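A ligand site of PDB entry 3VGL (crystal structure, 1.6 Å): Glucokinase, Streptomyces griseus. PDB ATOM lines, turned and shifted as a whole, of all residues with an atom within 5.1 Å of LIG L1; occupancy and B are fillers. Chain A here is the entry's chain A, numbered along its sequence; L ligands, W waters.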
ATOM      1  N   ASP A   8     -12.227  10.060 -24.523  1.00  0.00           N
ATOM      2  CA  ASP A   8     -11.142   9.552 -23.676  1.00  0.00           C
ATOM      3  C   ASP A   8     -11.748   9.267 -22.318  1.00  0.00           C
ATOM      4  O   ASP A   8     -12.263  10.177 -21.657  1.00  0.00           O
ATOM      5  CB  ASP A   8     -10.023  10.613 -23.582  1.00  0.00           C
ATOM      6  CG  ASP A   8      -8.810  10.120 -22.783  1.00  0.00           C
ATOM      7  OD1 ASP A   8      -8.971   9.591 -21.666  1.00  0.00           O
ATOM      8  OD2 ASP A   8      -7.670  10.289 -23.299  1.00  0.00           O
ATOM      9  N   GLY A  10     -10.893   8.139 -18.734  1.00  0.00           N
ATOM     10  CA  GLY A  10      -9.809   7.934 -17.761  1.00  0.00           C
ATOM     11  C   GLY A  10     -10.365   7.578 -16.402  1.00  0.00           C
ATOM     12  O   GLY A  10     -11.579   7.568 -16.190  1.00  0.00           O
ATOM     13  N   GLY A  11      -9.470   7.282 -15.458  1.00  0.00           N
ATOM     14  CA  GLY A  11      -9.869   6.971 -14.082  1.00  0.00           C
ATOM     15  C   GLY A  11     -10.650   8.102 -13.400  1.00  0.00           C
ATOM     16  O   GLY A  11     -11.464   7.836 -12.521  1.00  0.00           O
ATOM     17  N   THR A  12     -10.400   9.346 -13.814  1.00  0.00           N
ATOM     18  CA  THR A  12     -10.993  10.513 -13.162  1.00  0.00           C
ATOM     19  C   THR A  12     -11.998  11.196 -14.080  1.00  0.00           C
ATOM     20  O   THR A  12     -13.094  11.565 -13.635  1.00  0.00           O
ATOM     21  CB  THR A  12      -9.875  11.512 -12.710  1.00  0.00           C
ATOM     22  OG1 THR A  12      -8.972  10.825 -11.832  1.00  0.00           O
ATOM     23  CG2 THR A  12     -10.442  12.701 -11.951  1.00  0.00           C
ATOM     24  N   LYS A  13     -11.637  11.357 -15.354  1.00  0.00           N
ATOM     25  CA  LYS A  13     -12.385  12.208 -16.288  1.00  0.00           C
ATOM     26  C   LYS A  13     -12.750  11.497 -17.577  1.00  0.00           C
ATOM     27  O   LYS A  13     -11.979  10.693 -18.099  1.00  0.00           O
ATOM     28  CB  LYS A  13     -11.543  13.431 -16.681  1.00  0.00           C
ATOM     29  CG  LYS A  13     -10.955  14.236 -15.553  1.00  0.00           C
ATOM     30  CD  LYS A  13      -9.701  14.935 -16.042  1.00  0.00           C
ATOM     31  CE  LYS A  13      -9.038  15.715 -14.929  1.00  0.00           C
ATOM     32  NZ  LYS A  13      -7.885  16.502 -15.439  1.00  0.00           N
ATOM     33  N   THR A  33     -15.773  10.650 -14.541  1.00  0.00           N
ATOM     34  CA  THR A  33     -15.975   9.221 -14.736  1.00  0.00           C
ATOM     35  C   THR A  33     -16.779   8.644 -13.576  1.00  0.00           C
ATOM     36  O   THR A  33     -16.346   8.713 -12.432  1.00  0.00           O
ATOM     37  CB  THR A  33     -14.621   8.509 -14.871  1.00  0.00           C
ATOM     38  OG1 THR A  33     -13.861   9.216 -15.860  1.00  0.00           O
ATOM     39  CG2 THR A  33     -14.819   7.057 -15.281  1.00  0.00           C
ATOM     40  N   LEU A 130       0.755  10.593 -17.937  1.00  0.00           N
ATOM     41  CA  LEU A 130       0.745  10.717 -16.477  1.00  0.00           C
ATOM     42  C   LEU A 130      -0.585  11.309 -16.059  1.00  0.00           C
ATOM     43  O   LEU A 130      -0.862  12.470 -16.341  1.00  0.00           O
ATOM     44  CB  LEU A 130       1.890  11.650 -16.039  1.00  0.00           C
ATOM     45  CG  LEU A 130       3.310  11.189 -16.386  1.00  0.00           C
ATOM     46  CD1 LEU A 130       4.314  12.275 -16.014  1.00  0.00           C
ATOM     47  CD2 LEU A 130       3.646   9.860 -15.664  1.00  0.00           C
ATOM     48  N   GLY A 131      -1.379  10.510 -15.357  1.00  0.00           N
ATOM     49  CA  GLY A 131      -2.757  10.904 -14.996  1.00  0.00           C
ATOM     50  C   GLY A 131      -3.177  10.141 -13.770  1.00  0.00           C
ATOM     51  O   GLY A 131      -2.401  10.019 -12.805  1.00  0.00           O
ATOM     52  N   THR A 132      -4.399   9.611 -13.781  1.00  0.00           N
ATOM     53  CA  THR A 132      -4.836   8.742 -12.692  1.00  0.00           C
ATOM     54  C   THR A 132      -3.869   7.576 -12.533  1.00  0.00           C
ATOM     55  O   THR A 132      -3.537   7.175 -11.409  1.00  0.00           O
ATOM     56  CB  THR A 132      -6.229   8.197 -12.973  1.00  0.00           C
ATOM     57  OG1 THR A 132      -7.107   9.319 -13.109  1.00  0.00           O
ATOM     58  CG2 THR A 132      -6.745   7.345 -11.828  1.00  0.00           C
ATOM     59  N   GLY A 133      -3.454   7.053 -13.681  1.00  0.00           N
ATOM     60  CA  GLY A 133      -2.436   6.017 -13.750  1.00  0.00           C
ATOM     61  C   GLY A 133      -1.330   6.441 -14.714  1.00  0.00           C
ATOM     62  O   GLY A 133      -1.222   7.601 -15.086  1.00  0.00           O
ATOM     63  N   GLY A 181      -0.164  11.341 -11.999  1.00  0.00           N
ATOM     64  CA  GLY A 181      -0.771  12.512 -11.314  1.00  0.00           C
ATOM     65  C   GLY A 181      -1.131  12.178  -9.873  1.00  0.00           C
ATOM     66  O   GLY A 181      -0.950  12.990  -8.967  1.00  0.00           O
ATOM     67  N   ARG A 182      -1.623  10.955  -9.645  1.00  0.00           N
ATOM     68  CA  ARG A 182      -1.950  10.540  -8.281  1.00  0.00           C
ATOM     69  C   ARG A 182      -0.719  10.497  -7.392  1.00  0.00           C
ATOM     70  O   ARG A 182      -0.824  10.885  -6.234  1.00  0.00           O
ATOM     71  CB  ARG A 182      -2.698   9.199  -8.232  1.00  0.00           C
ATOM     72  CG  ARG A 182      -4.129   9.307  -8.580  1.00  0.00           C
ATOM     73  CD  ARG A 182      -4.875   8.034  -8.226  1.00  0.00           C
ATOM     74  NE  ARG A 182      -6.300   8.250  -8.444  1.00  0.00           N
ATOM     75  CZ  ARG A 182      -7.203   7.278  -8.472  1.00  0.00           C
ATOM     76  NH1 ARG A 182      -8.480   7.570  -8.692  1.00  0.00           N
ATOM     77  NH2 ARG A 182      -6.821   6.021  -8.302  1.00  0.00           N
ATOM     78  N   LEU A 184       2.026  12.329  -7.867  1.00  0.00           N
ATOM     79  CA  LEU A 184       2.322  13.746  -7.609  1.00  0.00           C
ATOM     80  C   LEU A 184       1.539  14.296  -6.405  1.00  0.00           C
ATOM     81  O   LEU A 184       2.120  14.936  -5.517  1.00  0.00           O
ATOM     82  CB  LEU A 184       2.043  14.578  -8.865  1.00  0.00           C
ATOM     83  CG  LEU A 184       2.326  16.093  -8.709  1.00  0.00           C
ATOM     84  CD1 LEU A 184       3.845  16.332  -8.600  1.00  0.00           C
ATOM     85  CD2 LEU A 184       1.738  16.768  -9.918  1.00  0.00           C
ATOM     86  N   VAL A 185       0.218  14.049  -6.401  1.00  0.00           N
ATOM     87  CA  VAL A 185      -0.625  14.492  -5.294  1.00  0.00           C
ATOM     88  C   VAL A 185      -0.172  13.876  -3.987  1.00  0.00           C
ATOM     89  O   VAL A 185      -0.094  14.551  -2.954  1.00  0.00           O
ATOM     90  CB  VAL A 185      -2.099  14.204  -5.595  1.00  0.00           C
ATOM     91  CG1 VAL A 185      -2.974  14.466  -4.376  1.00  0.00           C
ATOM     92  CG2 VAL A 185      -2.538  15.038  -6.777  1.00  0.00           C
ATOM     93  N   GLU A 214      -5.098  19.616  -4.537  1.00  0.00           N
ATOM     94  CA  GLU A 214      -5.423  19.011  -5.826  1.00  0.00           C
ATOM     95  C   GLU A 214      -4.259  19.149  -6.807  1.00  0.00           C
ATOM     96  O   GLU A 214      -3.441  20.061  -6.678  1.00  0.00           O
ATOM     97  CB  GLU A 214      -6.682  19.635  -6.414  1.00  0.00           C
ATOM     98  CG  GLU A 214      -7.945  19.331  -5.614  1.00  0.00           C
ATOM     99  CD  GLU A 214      -9.135  20.155  -6.047  1.00  0.00           C
ATOM    100  OE1 GLU A 214     -10.072  20.294  -5.222  1.00  0.00           O
ATOM    101  OE2 GLU A 214      -9.149  20.663  -7.188  1.00  0.00           O
ATOM    102  N   GLY A 215      -4.173  18.226  -7.777  1.00  0.00           N
ATOM    103  CA  GLY A 215      -3.068  18.253  -8.743  1.00  0.00           C
ATOM    104  C   GLY A 215      -2.818  19.630  -9.333  1.00  0.00           C
ATOM    105  O   GLY A 215      -1.690  20.114  -9.332  1.00  0.00           O
ATOM    106  N   LYS A 216      -3.862  20.272  -9.844  1.00  0.00           N
ATOM    107  CA  LYS A 216      -3.698  21.579 -10.486  1.00  0.00           C
ATOM    108  C   LYS A 216      -3.148  22.645  -9.528  1.00  0.00           C
ATOM    109  O   LYS A 216      -2.405  23.529  -9.946  1.00  0.00           O
ATOM    110  CB  LYS A 216      -5.006  22.025 -11.152  1.00  0.00           C
ATOM    111  CG  LYS A 216      -5.263  21.234 -12.452  1.00  0.00           C
ATOM    112  CD  LYS A 216      -6.636  21.459 -13.080  1.00  0.00           C
ATOM    113  CE  LYS A 216      -6.849  20.456 -14.221  1.00  0.00           C
ATOM    114  NZ  LYS A 216      -8.038  20.789 -15.064  1.00  0.00           N
ATOM    115  N   SER A 219       0.692  22.323  -9.483  1.00  0.00           N
ATOM    116  CA  SER A 219       1.276  22.927 -10.679  1.00  0.00           C
ATOM    117  C   SER A 219       1.358  24.445 -10.542  1.00  0.00           C
ATOM    118  O   SER A 219       2.442  25.030 -10.698  1.00  0.00           O
ATOM    119  CB  SER A 219       0.457  22.553 -11.911  1.00  0.00           C
ATOM    120  OG  SER A 219       0.633  21.163 -12.217  1.00  0.00           O
ATOM    121  N   PHE A 233       7.290  17.867  -7.662  1.00  0.00           N
ATOM    122  CA  PHE A 233       7.643  17.676  -9.060  1.00  0.00           C
ATOM    123  C   PHE A 233       8.995  17.015  -9.205  1.00  0.00           C
ATOM    124  O   PHE A 233       9.163  16.163 -10.092  1.00  0.00           O
ATOM    125  CB  PHE A 233       7.563  18.998  -9.845  1.00  0.00           C
ATOM    126  CG  PHE A 233       6.195  19.290 -10.353  1.00  0.00           C
ATOM    127  CD1 PHE A 233       5.413  20.264  -9.740  1.00  0.00           C
ATOM    128  CD2 PHE A 233       5.647  18.573 -11.420  1.00  0.00           C
ATOM    129  CE1 PHE A 233       4.127  20.545 -10.193  1.00  0.00           C
ATOM    130  CE2 PHE A 233       4.350  18.855 -11.881  1.00  0.00           C
ATOM    131  CZ  PHE A 233       3.581  19.838 -11.261  1.00  0.00           C
ATOM    132  N   GLY A 260      -0.937  12.986 -20.779  1.00  0.00           N
ATOM    133  CA  GLY A 260      -1.733  12.990 -19.551  1.00  0.00           C
ATOM    134  C   GLY A 260      -2.098  14.397 -19.166  1.00  0.00           C
ATOM    135  O   GLY A 260      -1.540  15.358 -19.699  1.00  0.00           O
ATOM    136  N   GLY A 261      -3.043  14.543 -18.237  1.00  0.00           N
ATOM    137  CA  GLY A 261      -3.422  15.877 -17.755  1.00  0.00           C
ATOM    138  C   GLY A 261      -2.278  16.749 -17.316  1.00  0.00           C
ATOM    139  O   GLY A 261      -2.269  17.929 -17.637  1.00  0.00           O
ATOM    140  N   VAL A 262      -1.300  16.202 -16.599  1.00  0.00           N
ATOM    141  CA  VAL A 262      -0.252  17.123 -16.120  1.00  0.00           C
ATOM    142  C   VAL A 262       0.662  17.633 -17.240  1.00  0.00           C
ATOM    143  O   VAL A 262       1.302  18.678 -17.088  1.00  0.00           O
ATOM    144  CB  VAL A 262       0.555  16.560 -14.959  1.00  0.00           C
ATOM    145  CG1 VAL A 262       1.327  15.352 -15.413  1.00  0.00           C
ATOM    146  CG2 VAL A 262       1.464  17.626 -14.322  1.00  0.00           C
ATOM    147  N   ASP A 264      -0.270  19.166 -19.641  1.00  0.00           N
ATOM    148  CA  ASP A 264      -0.788  20.500 -19.938  1.00  0.00           C
ATOM    149  C   ASP A 264       0.111  21.594 -19.380  1.00  0.00           C
ATOM    150  O   ASP A 264       0.057  22.757 -19.841  1.00  0.00           O
ATOM    151  CB  ASP A 264      -2.191  20.657 -19.332  1.00  0.00           C
ATOM    152  CG  ASP A 264      -3.239  19.872 -20.089  1.00  0.00           C
ATOM    153  OD1 ASP A 264      -3.067  19.612 -21.295  1.00  0.00           O
ATOM    154  OD2 ASP A 264      -4.274  19.548 -19.479  1.00  0.00           O
ATOM    155  N   GLU A 265       0.938  21.230 -18.401  1.00  0.00           N
ATOM    156  CA  GLU A 265       1.821  22.210 -17.766  1.00  0.00           C
ATOM    157  C   GLU A 265       3.127  22.478 -18.523  1.00  0.00           C
ATOM    158  O   GLU A 265       3.872  23.376 -18.134  1.00  0.00           O
ATOM    159  CB  GLU A 265       2.105  21.856 -16.306  1.00  0.00           C
ATOM    160  CG  GLU A 265       0.857  21.633 -15.460  1.00  0.00           C
ATOM    161  CD  GLU A 265      -0.030  22.865 -15.289  1.00  0.00           C
ATOM    162  OE1 GLU A 265       0.438  24.011 -15.512  1.00  0.00           O
ATOM    163  OE2 GLU A 265      -1.210  22.696 -14.918  1.00  0.00           O
HETATM  164  P1  LIG L   1      -7.585  10.829 -16.319  1.00  0.00           P
HETATM  165  O1  LIG L   1      -6.533   9.897 -15.702  1.00  0.00           O
HETATM  166  O2  LIG L   1      -8.993  10.644 -15.829  1.00  0.00           O
HETATM  167  N1  LIG L   1      -7.599  10.614 -18.018  1.00  0.00           N
HETATM  168  P2  LIG L   1      -5.846  13.148 -15.961  1.00  0.00           P
HETATM  169  O3  LIG L   1      -6.200  14.629 -15.845  1.00  0.00           O
HETATM  170  O4  LIG L   1      -4.981  12.660 -17.071  1.00  0.00           O
HETATM  171  O5  LIG L   1      -7.244  12.337 -15.919  1.00  0.00           O
HETATM  172  O6  LIG L   1      -5.161  12.648 -14.592  1.00  0.00           O
HETATM  173  C1  LIG L   1      -5.751  12.924 -13.310  1.00  0.00           C
HETATM  174  C2  LIG L   1      -4.659  12.955 -12.261  1.00  0.00           C
HETATM  175  O7  LIG L   1      -3.617  13.859 -12.659  1.00  0.00           O
HETATM  176  C3  LIG L   1      -5.208  13.470 -10.951  1.00  0.00           C
HETATM  177  O8  LIG L   1      -4.390  12.928  -9.905  1.00  0.00           O
HETATM  178  C4  LIG L   1      -4.950  14.953 -11.085  1.00  0.00           C
HETATM  179  O9  LIG L   1      -4.863  15.598  -9.829  1.00  0.00           O
HETATM  180  C5  LIG L   1      -3.637  15.027 -11.840  1.00  0.00           C
HETATM  181  N2  LIG L   1      -3.616  16.170 -12.776  1.00  0.00           N
HETATM  182  C6  LIG L   1      -4.378  16.353 -13.878  1.00  0.00           C
HETATM  183  N3  LIG L   1      -4.055  17.533 -14.489  1.00  0.00           N
HETATM  184  C7  LIG L   1      -3.052  18.069 -13.779  1.00  0.00           C
HETATM  185  C8  LIG L   1      -2.228  19.316 -13.822  1.00  0.00           C
HETATM  186  N4  LIG L   1      -2.396  20.225 -14.816  1.00  0.00           N
HETATM  187  N5  LIG L   1      -1.280  19.467 -12.878  1.00  0.00           N
HETATM  188  C9  LIG L   1      -1.061  18.581 -11.864  1.00  0.00           C
HETATM  189  N6  LIG L   1      -1.792  17.444 -11.761  1.00  0.00           N
HETATM  190  C10 LIG L   1      -2.761  17.176 -12.657  1.00  0.00           C
HETATM  191  C1  LG2 L   2      -3.994   1.320 -17.144  1.00  0.00           C
HETATM  192  C2  LG2 L   2      -3.679   1.651 -18.595  1.00  0.00           C
HETATM  193  C3  LG2 L   2      -3.994   3.111 -18.926  1.00  0.00           C
HETATM  194  C4  LG2 L   2      -3.306   3.985 -17.881  1.00  0.00           C
HETATM  195  C5  LG2 L   2      -3.582   5.475 -18.098  1.00  0.00           C
HETATM  196  C6  LG2 L   2      -3.262   2.320 -16.253  1.00  0.00           C
HETATM  197  O1  LG2 L   2      -3.593   2.128 -14.904  1.00  0.00           O
HETATM  198  O2  LG2 L   2      -3.467   0.013 -16.880  1.00  0.00           O
HETATM  199  O3  LG2 L   2      -4.394   0.823 -19.461  1.00  0.00           O
HETATM  200  O4  LG2 L   2      -3.469   3.436 -20.206  1.00  0.00           O
HETATM  201  O5  LG2 L   2      -3.705   3.630 -16.565  1.00  0.00           O
HETATM  202  O6  LG2 L   2      -4.980   5.743 -18.027  1.00  0.00           O
HETATM  203  O   HOH W   1      -6.453  14.559 -19.152  1.00  0.00           O
HETATM  204  O   HOH W   2      -5.599  13.044  -7.449  1.00  0.00           O
HETATM  205  O   HOH W   3      -2.066  14.344 -14.952  1.00  0.00           O
HETATM  206  O   HOH W   4      -4.955  19.048 -16.569  1.00  0.00           O
HETATM  207  O   HOH W   5      -6.564   7.111 -16.162  1.00  0.00           O
HETATM  208  O   HOH W   6      -9.875  11.433 -19.747  1.00  0.00           O
HETATM  209  O   HOH W   7      -6.888   9.003 -20.228  1.00  0.00           O
HETATM  210  O   HOH W   8      -4.361  10.797 -18.992  1.00  0.00           O
HETATM  211  O   HOH W   9      -6.374  18.457 -10.685  1.00  0.00           O
HETATM  212  O   HOH W  10      -6.361  16.123  -7.484  1.00  0.00           O
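The side-chain hydroxyl of Ser 219 sits at hydrogen-bond distance from a nitrogen (N5) of LIG L1 (2.6 Å).
The backbone NH (N) of Gly 215 sits close to an oxygen (O9) of LIG L1.
N4 of LIG L1 sits at hydrogen-bond distance from OE2 of Glu 265 (2.7 Å).
O2 of LIG L1 is in hydrogen-bond range of N of Gly 11 (3.4 Å).
An oxygen (O1) of LIG L1 lies within hydrogen-bond range of the side-chain hydroxyl (OG1) of Thr 132 (2.7 Å).
The backbone NH of Lys 13 sits at hydrogen-bond distance from an oxygen (O2) of LIG L1 (2.8 Å).
N of Thr 12 is in hydrogen-bond range of O2 of LIG L1.
O1 of LIG L1 sits at hydrogen-bond distance from N of Thr 132 (2.9 Å).
The side-chain amino group (NZ) of Lys 13 lies within salt-bridge range of an oxygen (O3) of LIG L1, 2.6 Å away.
The backbone NH (N) of Arg 182 sits at hydrogen-bond distance from an oxygen (O8) of LIG L1, at 3.4 Å.
N of Gly 261 is in hydrogen-bond range of O4 of LIG L1.
Merely in contact with LIG L1: Gly 131 (3.0 Å), Gly 181 (3.3 Å), Gly 10 (3.4 Å), Val 262 (3.6 Å), Lys 216 (3.8 Å), Leu 184 (3.9 Å), Val 185 (3.9 Å) and Gly 260 (3.96 Å).
Hydrophobic or aromatic side chains that line LIG L1: Leu 184, Val 185 and Val 262.
Of the 24 residues printed, 17 come within 4 Å of LIG L1.
The side-chain hydroxyl (OG1) of Thr 33 sits close to the backbone NH (N) of Lys 13 (3.1 Å).
The backbone NH (N) of Arg 182 sits at hydrogen-bond distance from the backbone carbonyl oxygen (O) of Gly 131.
The backbone carbonyl oxygen of Gly 131 lies within hydrogen-bond range of the backbone NH of Gly 181.
The backbone carbonyl oxygen (O) of Gly 10 is in hydrogen-bond range of the side-chain hydroxyl (OG1) of Thr 33 (2.8 Å).
The backbone carbonyl oxygen (O) of Thr 12 sits at hydrogen-bond distance from the backbone NH (N) of Thr 33, at 3.0 Å.
OG1 of Thr 12 sits at hydrogen-bond distance from OG1 of Thr 132 (2.7 Å).
Water W3 lies within hydrogen-bond range of the backbone NH of Val 262, the backbone carbonyl oxygen of Leu 130, an oxygen (O7) of LIG L1 and the backbone NH of Gly 261.
Water W5 lies within hydrogen-bond range of an oxygen (O6) of LG2 L2 (2.8 Å), an oxygen (O1) of LIG L1 (2.8 Å) and the backbone NH (N) of Gly 11 (3.0 Å).
Water W7 bridges OD1 of Asp 8 and N1 of LIG L1.
Water W10 bridges an oxygen (O9) of LIG L1 (2.8 Å) and the backbone NH of Gly 215 (3.0 Å).
Water W6 lies within hydrogen-bond range of the backbone carbonyl oxygen of Lys 13 (2.8 Å), the side-chain carboxylate of Asp 8 (2.8 Å) and a nitrogen (N1) of LIG L1 (3.0 Å).
Water W9 lies within hydrogen-bond range of N of Lys 216 (3.2 Å) and O9 of LIG L1 (3.3 Å).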
